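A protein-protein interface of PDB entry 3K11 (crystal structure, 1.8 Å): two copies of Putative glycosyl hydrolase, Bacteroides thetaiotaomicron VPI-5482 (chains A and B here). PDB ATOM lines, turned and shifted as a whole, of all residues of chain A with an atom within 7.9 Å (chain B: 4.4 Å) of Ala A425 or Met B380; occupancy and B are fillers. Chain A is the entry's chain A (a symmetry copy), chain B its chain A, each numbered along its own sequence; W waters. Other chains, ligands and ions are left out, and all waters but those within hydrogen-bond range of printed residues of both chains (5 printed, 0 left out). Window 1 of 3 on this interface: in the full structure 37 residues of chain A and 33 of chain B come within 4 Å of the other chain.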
ATOM      1  N   LEU A  15      27.780   8.747   0.859  1.00  0.00           N
ATOM      2  CA  LEU A  15      26.931   9.802   1.386  1.00  0.00           C
ATOM      3  C   LEU A  15      25.440   9.574   1.052  1.00  0.00           C
ATOM      4  O   LEU A  15      24.631  10.413   1.416  1.00  0.00           O
ATOM      5  CB  LEU A  15      27.457  11.198   0.942  1.00  0.00           C
ATOM      6  CG  LEU A  15      28.680  11.742   1.749  1.00  0.00           C
ATOM      7  CD1 LEU A  15      29.426  12.843   0.987  1.00  0.00           C
ATOM      8  CD2 LEU A  15      28.365  12.237   3.220  1.00  0.00           C
ATOM      9  N   TYR A  20      16.441   4.350   6.944  1.00  0.00           N
ATOM     10  CA  TYR A  20      16.058   4.052   8.348  1.00  0.00           C
ATOM     11  C   TYR A  20      14.577   3.849   8.454  1.00  0.00           C
ATOM     12  O   TYR A  20      13.836   4.518   7.784  1.00  0.00           O
ATOM     13  CB  TYR A  20      16.462   5.206   9.292  1.00  0.00           C
ATOM     14  CG  TYR A  20      17.962   5.465   9.326  1.00  0.00           C
ATOM     15  CD1 TYR A  20      18.833   4.547   9.933  1.00  0.00           C
ATOM     16  CD2 TYR A  20      18.521   6.613   8.751  1.00  0.00           C
ATOM     17  CE1 TYR A  20      20.221   4.769   9.979  1.00  0.00           C
ATOM     18  CE2 TYR A  20      19.911   6.828   8.769  1.00  0.00           C
ATOM     19  CZ  TYR A  20      20.745   5.908   9.387  1.00  0.00           C
ATOM     20  OH  TYR A  20      22.115   6.054   9.421  1.00  0.00           O
ATOM     21  N   TYR A  24      16.784   9.124  12.685  1.00  0.00           N
ATOM     22  CA  TYR A  24      18.207   9.011  12.987  1.00  0.00           C
ATOM     23  C   TYR A  24      18.826  10.395  12.812  1.00  0.00           C
ATOM     24  O   TYR A  24      18.340  11.196  12.051  1.00  0.00           O
ATOM     25  CB  TYR A  24      18.911   8.029  12.018  1.00  0.00           C
ATOM     26  CG  TYR A  24      20.373   7.822  12.376  1.00  0.00           C
ATOM     27  CD1 TYR A  24      20.753   6.878  13.336  1.00  0.00           C
ATOM     28  CD2 TYR A  24      21.366   8.631  11.833  1.00  0.00           C
ATOM     29  CE1 TYR A  24      22.075   6.765  13.714  1.00  0.00           C
ATOM     30  CE2 TYR A  24      22.709   8.483  12.194  1.00  0.00           C
ATOM     31  CZ  TYR A  24      23.044   7.573  13.156  1.00  0.00           C
ATOM     32  OH  TYR A  24      24.340   7.432  13.540  1.00  0.00           O
ATOM     33  N   GLY A  25      19.861  10.698  13.588  1.00  0.00           N
ATOM     34  CA  GLY A  25      20.659  11.882  13.323  1.00  0.00           C
ATOM     35  C   GLY A  25      20.412  13.008  14.303  1.00  0.00           C
ATOM     36  O   GLY A  25      20.214  12.795  15.504  1.00  0.00           O
ATOM     37  N   ASP A  26      20.413  14.201  13.752  1.00  0.00           N
ATOM     38  CA  ASP A  26      20.251  15.414  14.539  1.00  0.00           C
ATOM     39  C   ASP A  26      19.004  15.375  15.402  1.00  0.00           C
ATOM     40  O   ASP A  26      17.966  14.851  14.996  1.00  0.00           O
ATOM     41  CB  ASP A  26      20.143  16.630  13.619  1.00  0.00           C
ATOM     42  CG  ASP A  26      21.456  16.971  12.892  1.00  0.00           C
ATOM     43  OD1 ASP A  26      22.555  16.618  13.345  1.00  0.00           O
ATOM     44  OD2 ASP A  26      21.354  17.644  11.847  1.00  0.00           O
ATOM     45  N   ILE A 348      31.873  10.551  24.100  1.00  0.00           N
ATOM     46  CA  ILE A 348      32.108  10.148  22.716  1.00  0.00           C
ATOM     47  C   ILE A 348      31.546   8.726  22.532  1.00  0.00           C
ATOM     48  O   ILE A 348      30.843   8.394  21.532  1.00  0.00           O
ATOM     49  CB  ILE A 348      33.615  10.179  22.342  1.00  0.00           C
ATOM     50  CG1 ILE A 348      34.143  11.618  22.264  1.00  0.00           C
ATOM     51  CG2 ILE A 348      33.818   9.478  21.002  1.00  0.00           C
ATOM     52  CD1 ILE A 348      35.695  11.763  22.203  1.00  0.00           C
ATOM     53  N   PRO A 352      26.024   8.901  21.386  1.00  0.00           N
ATOM     54  CA  PRO A 352      25.234   8.400  20.253  1.00  0.00           C
ATOM     55  C   PRO A 352      24.287   7.250  20.571  1.00  0.00           C
ATOM     56  O   PRO A 352      23.247   7.103  19.902  1.00  0.00           O
ATOM     57  CB  PRO A 352      26.311   7.989  19.257  1.00  0.00           C
ATOM     58  CG  PRO A 352      27.468   8.857  19.585  1.00  0.00           C
ATOM     59  CD  PRO A 352      27.468   8.827  21.098  1.00  0.00           C
ATOM     60  N   PRO A 419      26.867  17.599  19.860  1.00  0.00           N
ATOM     61  CA  PRO A 419      26.856  16.542  18.866  1.00  0.00           C
ATOM     62  C   PRO A 419      26.631  17.085  17.468  1.00  0.00           C
ATOM     63  O   PRO A 419      26.017  18.147  17.308  1.00  0.00           O
ATOM     64  CB  PRO A 419      25.689  15.661  19.306  1.00  0.00           C
ATOM     65  CG  PRO A 419      24.828  16.531  20.090  1.00  0.00           C
ATOM     66  CD  PRO A 419      25.715  17.519  20.758  1.00  0.00           C
ATOM     67  N   GLN A 420      27.140  16.357  16.473  1.00  0.00           N
ATOM     68  CA  GLN A 420      27.087  16.753  15.104  1.00  0.00           C
ATOM     69  C   GLN A 420      27.284  15.528  14.220  1.00  0.00           C
ATOM     70  O   GLN A 420      27.995  14.583  14.562  1.00  0.00           O
ATOM     71  CB  GLN A 420      28.194  17.801  14.872  1.00  0.00           C
ATOM     72  CG  GLN A 420      28.311  18.309  13.485  1.00  0.00           C
ATOM     73  CD  GLN A 420      29.061  19.630  13.388  1.00  0.00           C
ATOM     74  OE1 GLN A 420      29.387  20.258  14.404  1.00  0.00           O
ATOM     75  NE2 GLN A 420      29.366  20.045  12.147  1.00  0.00           N
ATOM     76  N   MET A 421      26.646  15.549  13.063  1.00  0.00           N
ATOM     77  CA  MET A 421      26.801  14.481  12.105  1.00  0.00           C
ATOM     78  C   MET A 421      28.202  14.591  11.492  1.00  0.00           C
ATOM     79  O   MET A 421      28.687  15.682  11.160  1.00  0.00           O
ATOM     80  CB  MET A 421      25.700  14.591  11.031  1.00  0.00           C
ATOM     81  CG  MET A 421      24.277  14.318  11.573  1.00  0.00           C
ATOM     82  SD  MET A 421      24.043  12.456  11.787  1.00  0.00           S
ATOM     83  CE  MET A 421      23.892  11.918  10.021  1.00  0.00           C
ATOM     84  N   ASN A 422      28.863  13.455  11.370  1.00  0.00           N
ATOM     85  CA  ASN A 422      30.174  13.365  10.744  1.00  0.00           C
ATOM     86  C   ASN A 422      30.200  12.067   9.958  1.00  0.00           C
ATOM     87  O   ASN A 422      30.055  10.999  10.525  1.00  0.00           O
ATOM     88  CB  ASN A 422      31.270  13.407  11.810  1.00  0.00           C
ATOM     89  CG  ASN A 422      32.630  13.621  11.225  1.00  0.00           C
ATOM     90  OD1 ASN A 422      32.866  13.332  10.049  1.00  0.00           O
ATOM     91  ND2 ASN A 422      33.547  14.118  12.040  1.00  0.00           N
ATOM     92  N   ASP A 423      30.368  12.150   8.646  1.00  0.00           N
ATOM     93  CA  ASP A 423      30.383  10.915   7.836  1.00  0.00           C
ATOM     94  C   ASP A 423      29.088  10.101   8.042  1.00  0.00           C
ATOM     95  O   ASP A 423      29.111   8.893   8.026  1.00  0.00           O
ATOM     96  CB  ASP A 423      31.644  10.128   8.231  1.00  0.00           C
ATOM     97  CG  ASP A 423      32.302   9.420   7.101  1.00  0.00           C
ATOM     98  OD1 ASP A 423      31.820   9.454   5.954  1.00  0.00           O
ATOM     99  OD2 ASP A 423      33.321   8.807   7.407  1.00  0.00           O
ATOM    100  N   SER A 424      27.948  10.799   8.211  1.00  0.00           N
ATOM    101  CA  SER A 424      26.623  10.208   8.277  1.00  0.00           C
ATOM    102  C   SER A 424      26.320   9.538   9.602  1.00  0.00           C
ATOM    103  O   SER A 424      25.287   8.870   9.720  1.00  0.00           O
ATOM    104  CB  SER A 424      26.406   9.186   7.132  1.00  0.00           C
ATOM    105  OG  SER A 424      26.575   9.768   5.853  1.00  0.00           O
ATOM    106  N   ALA A 425      27.209   9.698  10.586  1.00  0.00           N
ATOM    107  CA  ALA A 425      27.035   9.123  11.941  1.00  0.00           C
ATOM    108  C   ALA A 425      26.941  10.255  12.972  1.00  0.00           C
ATOM    109  O   ALA A 425      27.655  11.240  12.878  1.00  0.00           O
ATOM    110  CB  ALA A 425      28.248   8.210  12.299  1.00  0.00           C
ATOM    111  N   VAL A 426      26.107  10.063  13.993  1.00  0.00           N
ATOM    112  CA  VAL A 426      26.059  10.983  15.118  1.00  0.00           C
ATOM    113  C   VAL A 426      27.364  10.883  15.890  1.00  0.00           C
ATOM    114  O   VAL A 426      27.777   9.779  16.262  1.00  0.00           O
ATOM    115  CB  VAL A 426      24.887  10.641  16.041  1.00  0.00           C
ATOM    116  CG1 VAL A 426      24.963  11.448  17.343  1.00  0.00           C
ATOM    117  CG2 VAL A 426      23.532  10.847  15.321  1.00  0.00           C
ATOM    118  N   GLN A 427      28.058  12.019  16.075  1.00  0.00           N
ATOM    119  CA  GLN A 427      29.249  12.077  16.906  1.00  0.00           C
ATOM    120  C   GLN A 427      29.120  13.141  17.960  1.00  0.00           C
ATOM    121  O   GLN A 427      28.583  14.210  17.703  1.00  0.00           O
ATOM    122  CB  GLN A 427      30.497  12.307  16.055  1.00  0.00           C
ATOM    123  CG  GLN A 427      30.865  11.103  15.180  1.00  0.00           C
ATOM    124  CD  GLN A 427      31.505   9.946  15.959  1.00  0.00           C
ATOM    125  OE1 GLN A 427      31.998  10.143  17.068  1.00  0.00           O
ATOM    126  NE2 GLN A 427      31.597   8.758  15.335  1.00  0.00           N
ATOM    127  N   TYR A 428      29.605  12.838  19.164  1.00  0.00           N
ATOM    128  CA  TYR A 428      29.562  13.784  20.277  1.00  0.00           C
ATOM    129  C   TYR A 428      30.846  14.571  20.399  1.00  0.00           C
ATOM    130  O   TYR A 428      31.924  13.980  20.475  1.00  0.00           O
ATOM    131  CB  TYR A 428      29.199  13.073  21.594  1.00  0.00           C
ATOM    132  CG  TYR A 428      27.713  13.117  21.850  1.00  0.00           C
ATOM    133  CD1 TYR A 428      26.811  12.551  20.953  1.00  0.00           C
ATOM    134  CD2 TYR A 428      27.190  13.768  22.954  1.00  0.00           C
ATOM    135  CE1 TYR A 428      25.438  12.648  21.154  1.00  0.00           C
ATOM    136  CE2 TYR A 428      25.828  13.856  23.170  1.00  0.00           C
ATOM    137  CZ  TYR A 428      24.929  13.306  22.241  1.00  0.00           C
ATOM    138  OH  TYR A 428      23.541  13.380  22.440  1.00  0.00           O
ATOM    139  N   TYR A 429      30.723  15.894  20.487  1.00  0.00           N
ATOM    140  CA  TYR A 429      31.877  16.794  20.614  1.00  0.00           C
ATOM    141  C   TYR A 429      31.682  17.643  21.872  1.00  0.00           C
ATOM    142  O   TYR A 429      30.605  18.103  22.140  1.00  0.00           O
ATOM    143  CB  TYR A 429      32.029  17.685  19.360  1.00  0.00           C
ATOM    144  CG  TYR A 429      32.299  16.836  18.139  1.00  0.00           C
ATOM    145  CD1 TYR A 429      33.573  16.326  17.895  1.00  0.00           C
ATOM    146  CD2 TYR A 429      31.287  16.486  17.276  1.00  0.00           C
ATOM    147  CE1 TYR A 429      33.820  15.499  16.826  1.00  0.00           C
ATOM    148  CE2 TYR A 429      31.532  15.655  16.200  1.00  0.00           C
ATOM    149  CZ  TYR A 429      32.791  15.146  15.987  1.00  0.00           C
ATOM    150  OH  TYR A 429      33.033  14.298  14.921  1.00  0.00           O
ATOM    151  N   PRO A 438      30.110  17.843   5.867  1.00  0.00           N
ATOM    152  CA  PRO A 438      29.546  16.545   6.278  1.00  0.00           C
ATOM    153  C   PRO A 438      30.532  15.583   6.909  1.00  0.00           C
ATOM    154  O   PRO A 438      30.111  14.678   7.634  1.00  0.00           O
ATOM    155  CB  PRO A 438      29.099  15.926   4.951  1.00  0.00           C
ATOM    156  CG  PRO A 438      29.013  17.003   4.027  1.00  0.00           C
ATOM    157  CD  PRO A 438      29.946  18.065   4.424  1.00  0.00           C
ATOM    158  N   PHE A 440      34.559  15.604   8.596  1.00  0.00           N
ATOM    159  CA  PHE A 440      35.613  16.479   9.063  1.00  0.00           C
ATOM    160  C   PHE A 440      36.446  15.862  10.184  1.00  0.00           C
ATOM    161  O   PHE A 440      35.983  14.953  10.906  1.00  0.00           O
ATOM    162  CB  PHE A 440      35.011  17.798   9.578  1.00  0.00           C
ATOM    163  CG  PHE A 440      34.097  17.632  10.761  1.00  0.00           C
ATOM    164  CD1 PHE A 440      32.749  17.396  10.576  1.00  0.00           C
ATOM    165  CD2 PHE A 440      34.587  17.706  12.062  1.00  0.00           C
ATOM    166  CE1 PHE A 440      31.902  17.229  11.659  1.00  0.00           C
ATOM    167  CE2 PHE A 440      33.741  17.550  13.167  1.00  0.00           C
ATOM    168  CZ  PHE A 440      32.406  17.289  12.978  1.00  0.00           C
ATOM    169  N   PRO B 194      36.658  10.558  13.136  1.00  0.00           N
ATOM    170  CA  PRO B 194      35.716  11.632  13.542  1.00  0.00           C
ATOM    171  C   PRO B 194      36.055  12.329  14.841  1.00  0.00           C
ATOM    172  O   PRO B 194      35.334  13.254  15.237  1.00  0.00           O
ATOM    173  CB  PRO B 194      34.389  10.886  13.653  1.00  0.00           C
ATOM    174  CG  PRO B 194      34.779   9.514  14.086  1.00  0.00           C
ATOM    175  CD  PRO B 194      36.060   9.223  13.321  1.00  0.00           C
ATOM    176  N   THR B 198      42.061   8.945  16.693  1.00  0.00           N
ATOM    177  CA  THR B 198      41.220   7.766  16.444  1.00  0.00           C
ATOM    178  C   THR B 198      41.946   6.763  15.576  1.00  0.00           C
ATOM    179  O   THR B 198      42.536   7.101  14.551  1.00  0.00           O
ATOM    180  CB  THR B 198      39.914   8.191  15.715  1.00  0.00           C
ATOM    181  OG1 THR B 198      39.223   9.161  16.519  1.00  0.00           O
ATOM    182  CG2 THR B 198      39.022   7.019  15.474  1.00  0.00           C
ATOM    183  N   LEU B 199      41.878   5.501  15.997  1.00  0.00           N
ATOM    184  CA  LEU B 199      42.324   4.411  15.183  1.00  0.00           C
ATOM    185  C   LEU B 199      41.114   3.834  14.445  1.00  0.00           C
ATOM    186  O   LEU B 199      40.100   3.586  15.056  1.00  0.00           O
ATOM    187  CB  LEU B 199      43.002   3.331  15.995  1.00  0.00           C
ATOM    188  CG  LEU B 199      44.285   3.667  16.758  1.00  0.00           C
ATOM    189  CD1 LEU B 199      44.829   2.397  17.492  1.00  0.00           C
ATOM    190  CD2 LEU B 199      45.355   4.318  15.799  1.00  0.00           C
ATOM    191  N   TRP B 200      41.309   3.598  13.152  1.00  0.00           N
ATOM    192  CA  TRP B 200      40.358   2.917  12.268  1.00  0.00           C
ATOM    193  C   TRP B 200      40.899   1.556  11.951  1.00  0.00           C
ATOM    194  O   TRP B 200      42.032   1.426  11.475  1.00  0.00           O
ATOM    195  CB  TRP B 200      40.243   3.689  10.967  1.00  0.00           C
ATOM    196  CG  TRP B 200      39.475   4.953  11.056  1.00  0.00           C
ATOM    197  CD1 TRP B 200      39.735   6.047  11.842  1.00  0.00           C
ATOM    198  CD2 TRP B 200      38.355   5.281  10.260  1.00  0.00           C
ATOM    199  NE1 TRP B 200      38.813   7.026  11.597  1.00  0.00           N
ATOM    200  CE2 TRP B 200      37.961   6.598  10.614  1.00  0.00           C
ATOM    201  CE3 TRP B 200      37.636   4.588   9.274  1.00  0.00           C
ATOM    202  CZ2 TRP B 200      36.887   7.255   9.997  1.00  0.00           C
ATOM    203  CZ3 TRP B 200      36.547   5.217   8.686  1.00  0.00           C
ATOM    204  CH2 TRP B 200      36.197   6.555   9.028  1.00  0.00           C
ATOM    205  N   HIS B 250      35.694  -1.853  15.066  1.00  0.00           N
ATOM    206  CA  HIS B 250      35.958  -0.961  13.920  1.00  0.00           C
ATOM    207  C   HIS B 250      36.751   0.281  14.319  1.00  0.00           C
ATOM    208  O   HIS B 250      37.578   0.762  13.560  1.00  0.00           O
ATOM    209  CB  HIS B 250      34.647  -0.524  13.251  1.00  0.00           C
ATOM    210  CG  HIS B 250      34.838   0.250  11.993  1.00  0.00           C
ATOM    211  ND1 HIS B 250      33.893   1.147  11.510  1.00  0.00           N
ATOM    212  CD2 HIS B 250      35.865   0.265  11.116  1.00  0.00           C
ATOM    213  CE1 HIS B 250      34.340   1.667  10.373  1.00  0.00           C
ATOM    214  NE2 HIS B 250      35.535   1.151  10.107  1.00  0.00           N
ATOM    215  N   GLY B 251      36.484   0.794  15.520  1.00  0.00           N
ATOM    216  CA  GLY B 251      37.135   2.021  15.928  1.00  0.00           C
ATOM    217  C   GLY B 251      37.601   2.057  17.353  1.00  0.00           C
ATOM    218  O   GLY B 251      37.137   1.315  18.245  1.00  0.00           O
ATOM    219  N   GLY B 379      31.963   5.045   7.240  1.00  0.00           N
ATOM    220  CA  GLY B 379      32.829   5.601   8.263  1.00  0.00           C
ATOM    221  C   GLY B 379      32.557   4.966   9.629  1.00  0.00           C
ATOM    222  O   GLY B 379      32.060   3.837   9.721  1.00  0.00           O
ATOM    223  N   MET B 380      32.848   5.715  10.685  1.00  0.00           N
ATOM    224  CA  MET B 380      32.817   5.195  12.061  1.00  0.00           C
ATOM    225  C   MET B 380      31.657   5.740  12.846  1.00  0.00           C
ATOM    226  O   MET B 380      31.410   6.943  12.850  1.00  0.00           O
ATOM    227  CB  MET B 380      34.111   5.592  12.774  1.00  0.00           C
ATOM    228  CG  MET B 380      34.257   4.988  14.192  1.00  0.00           C
ATOM    229  SD  MET B 380      35.879   5.509  15.027  1.00  0.00           S
ATOM    230  CE  MET B 380      37.071   4.620  13.678  1.00  0.00           C
ATOM    231  N   ALA B 381      30.949   4.872  13.540  1.00  0.00           N
ATOM    232  CA  ALA B 381      29.857   5.296  14.395  1.00  0.00           C
ATOM    233  C   ALA B 381      30.035   4.671  15.797  1.00  0.00           C
ATOM    234  O   ALA B 381      30.773   3.660  15.977  1.00  0.00           O
ATOM    235  CB  ALA B 381      28.483   4.853  13.802  1.00  0.00           C
ATOM    236  N   PHE B 382      29.285   5.222  16.745  1.00  0.00           N
ATOM    237  CA  PHE B 382      29.152   4.645  18.055  1.00  0.00           C
ATOM    238  C   PHE B 382      27.698   4.294  18.399  1.00  0.00           C
ATOM    239  O   PHE B 382      27.270   4.319  19.542  1.00  0.00           O
ATOM    240  CB  PHE B 382      29.822   5.545  19.098  1.00  0.00           C
ATOM    241  CG  PHE B 382      31.291   5.548  18.945  1.00  0.00           C
ATOM    242  CD1 PHE B 382      32.013   4.402  19.237  1.00  0.00           C
ATOM    243  CD2 PHE B 382      31.943   6.618  18.417  1.00  0.00           C
ATOM    244  CE1 PHE B 382      33.366   4.344  19.013  1.00  0.00           C
ATOM    245  CE2 PHE B 382      33.272   6.559  18.210  1.00  0.00           C
ATOM    246  CZ  PHE B 382      33.983   5.443  18.524  1.00  0.00           C
ATOM    247  N   PHE B 386      23.512   3.103  12.523  1.00  0.00           N
ATOM    248  CA  PHE B 386      24.381   3.506  11.426  1.00  0.00           C
ATOM    249  C   PHE B 386      24.865   2.275  10.654  1.00  0.00           C
ATOM    250  O   PHE B 386      24.729   2.189   9.425  1.00  0.00           O
ATOM    251  CB  PHE B 386      25.555   4.310  11.984  1.00  0.00           C
ATOM    252  CG  PHE B 386      26.639   4.601  10.972  1.00  0.00           C
ATOM    253  CD1 PHE B 386      26.521   5.664  10.110  1.00  0.00           C
ATOM    254  CD2 PHE B 386      27.748   3.787  10.867  1.00  0.00           C
ATOM    255  CE1 PHE B 386      27.491   5.932   9.203  1.00  0.00           C
ATOM    256  CE2 PHE B 386      28.756   4.104   9.970  1.00  0.00           C
ATOM    257  CZ  PHE B 386      28.589   5.153   9.128  1.00  0.00           C
ATOM    258  N   TYR B 387      25.366   1.289  11.381  1.00  0.00           N
ATOM    259  CA  TYR B 387      25.940   0.107  10.706  1.00  0.00           C
ATOM    260  C   TYR B 387      24.862  -0.759  10.067  1.00  0.00           C
ATOM    261  O   TYR B 387      25.028  -1.288   8.973  1.00  0.00           O
ATOM    262  CB  TYR B 387      26.797  -0.704  11.662  1.00  0.00           C
ATOM    263  CG  TYR B 387      28.112  -0.036  12.025  1.00  0.00           C
ATOM    264  CD1 TYR B 387      29.182  -0.039  11.138  1.00  0.00           C
ATOM    265  CD2 TYR B 387      28.279   0.635  13.237  1.00  0.00           C
ATOM    266  CE1 TYR B 387      30.370   0.603  11.439  1.00  0.00           C
ATOM    267  CE2 TYR B 387      29.478   1.267  13.551  1.00  0.00           C
ATOM    268  CZ  TYR B 387      30.532   1.243  12.655  1.00  0.00           C
ATOM    269  OH  TYR B 387      31.731   1.855  12.952  1.00  0.00           O
HETATM  270  O   HOH W   1      23.672   4.185   7.833  1.00  0.00           O
HETATM  271  O   HOH W   2      27.364   7.171  15.988  1.00  0.00           O
HETATM  272  O   HOH W   3      31.877   9.386  11.895  1.00  0.00           O
HETATM  273  O   HOH W   4      33.871   8.689  10.223  1.00  0.00           O
HETATM  274  O   HOH W   5      29.827   6.739   6.307  1.00  0.00           O
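The side-chain amide nitrogen (NE2) of Gln A427 sits at hydrogen-bond distance from the backbone carbonyl oxygen (O) of Met B380, 3.1 Å away. OH of Tyr A429 is in hydrogen-bond range of O of Pro B194 (2.5 Å).
The side-chain hydroxyl of Tyr A24 sits at hydrogen-bond distance from the backbone NH of Val A426, at 3.2 Å. The backbone NH (N) of Ala B381 is in hydrogen-bond range of the side-chain hydroxyl (OH) of Tyr B387. The side-chain amide nitrogen of Asn A422 lies within hydrogen-bond range of the backbone carbonyl oxygen of Phe A440. The side-chain amide nitrogen (ND2) of Asn A422 sits at hydrogen-bond distance from the side-chain hydroxyl (OH) of Tyr A429 (2.9 Å). The backbone NH (N) of Gln A420 sits at hydrogen-bond distance from the backbone carbonyl oxygen (O) of Gln A427 (2.9 Å). O of Pro A438 lies within hydrogen-bond range of N of Asp A423 (2.7 Å).
Among the printed residues, pairs that only touch across the chains: Tyr A20 with Phe B386, Tyr A24 with Phe B386, Ile A348 with Phe B382, Pro A352 with Phe B382, Asn A422 with Pro B194, Asp A423 with Trp B200, Asp A423 with Gly B379, Asp A423 with Phe B386, Ser A424 with Phe B386, Ala A425 with Met B380, Ala A425 with Ala B381, Ala A425 with Phe B386, Gln A427 with Pro B194, Gln A427 with Ala B381 and Gln A427 with Phe B382.
Ala A425 touches just these residues of chain B: Met B380 (3.5 Å), Ala B381 (3.7 Å) and Phe B386 (3.8 Å). Met B380 touches just these residues of chain A: Ala A425 (3.5 Å) and Gln A427 (3.1 Å). Gly B379 touches one residue of chain A. Of the printed residues of chain B, Asn A422 touches Pro B194. Printed residues of chain A within 4 Å of Ala B381: Ala A425 (3.7 Å) and Gln A427 (3.99 Å). Of the printed residues of chain B, Ile A348 touches Phe B382 (3.8 Å). The nearest printed residue of chain B that does not touch Ala A425 is Phe B382 (5.5 Å). The nearest printed residue of chain B that does not touch Ser A424 is Ala B381 (6.6 Å).
Printed residues of chain A that touch a printed residue of chain B: Tyr A20, Tyr A24, Ile A348, Pro A352, Asn A422, Asp A423, Ser A424, Ala A425, Gln A427 and Tyr A429. Of the 12 printed residues of chain B, 7 touch a printed residue of chain A. Printed residues of chain B that touch a printed residue of chain A: Pro B194, Trp B200, Gly B379, Met B380, Ala B381, Phe B382 and Phe B386. Hydrophobic or aromatic side chains of chain B that line the printed part of chain A: Pro B194, Trp B200, Ala B381, Phe B382 and Phe B386. Among the printed residues, no Asp or Glu carboxylate lies within 4 Å of a Lys or Arg side-chain nitrogen of the other chain.
No position is printed for both chains. Of the 17 pairs that touch across the chains among the printed residues, none has its exchanged pair printed and touching as well.
Water W2 lies within hydrogen-bond range of O of Val A426 (2.7 Å) and N of Phe B382 (2.8 Å). Water W3 bridges O of Met B380 (2.7 Å) and O of Asn A422 (2.8 Å). Water W1 bridges O of Phe B386 (2.8 Å) and OH of Tyr A20 (2.9 Å). Water W5 bridges O of Asp A423 (2.8 Å) and N of Gly B379 (2.9 Å). Water W4 lies within hydrogen-bond range of the side-chain carboxylate (OD2) of Asp A423 (2.9 Å) and the backbone NH (N) of Met B380 (3.2 Å).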
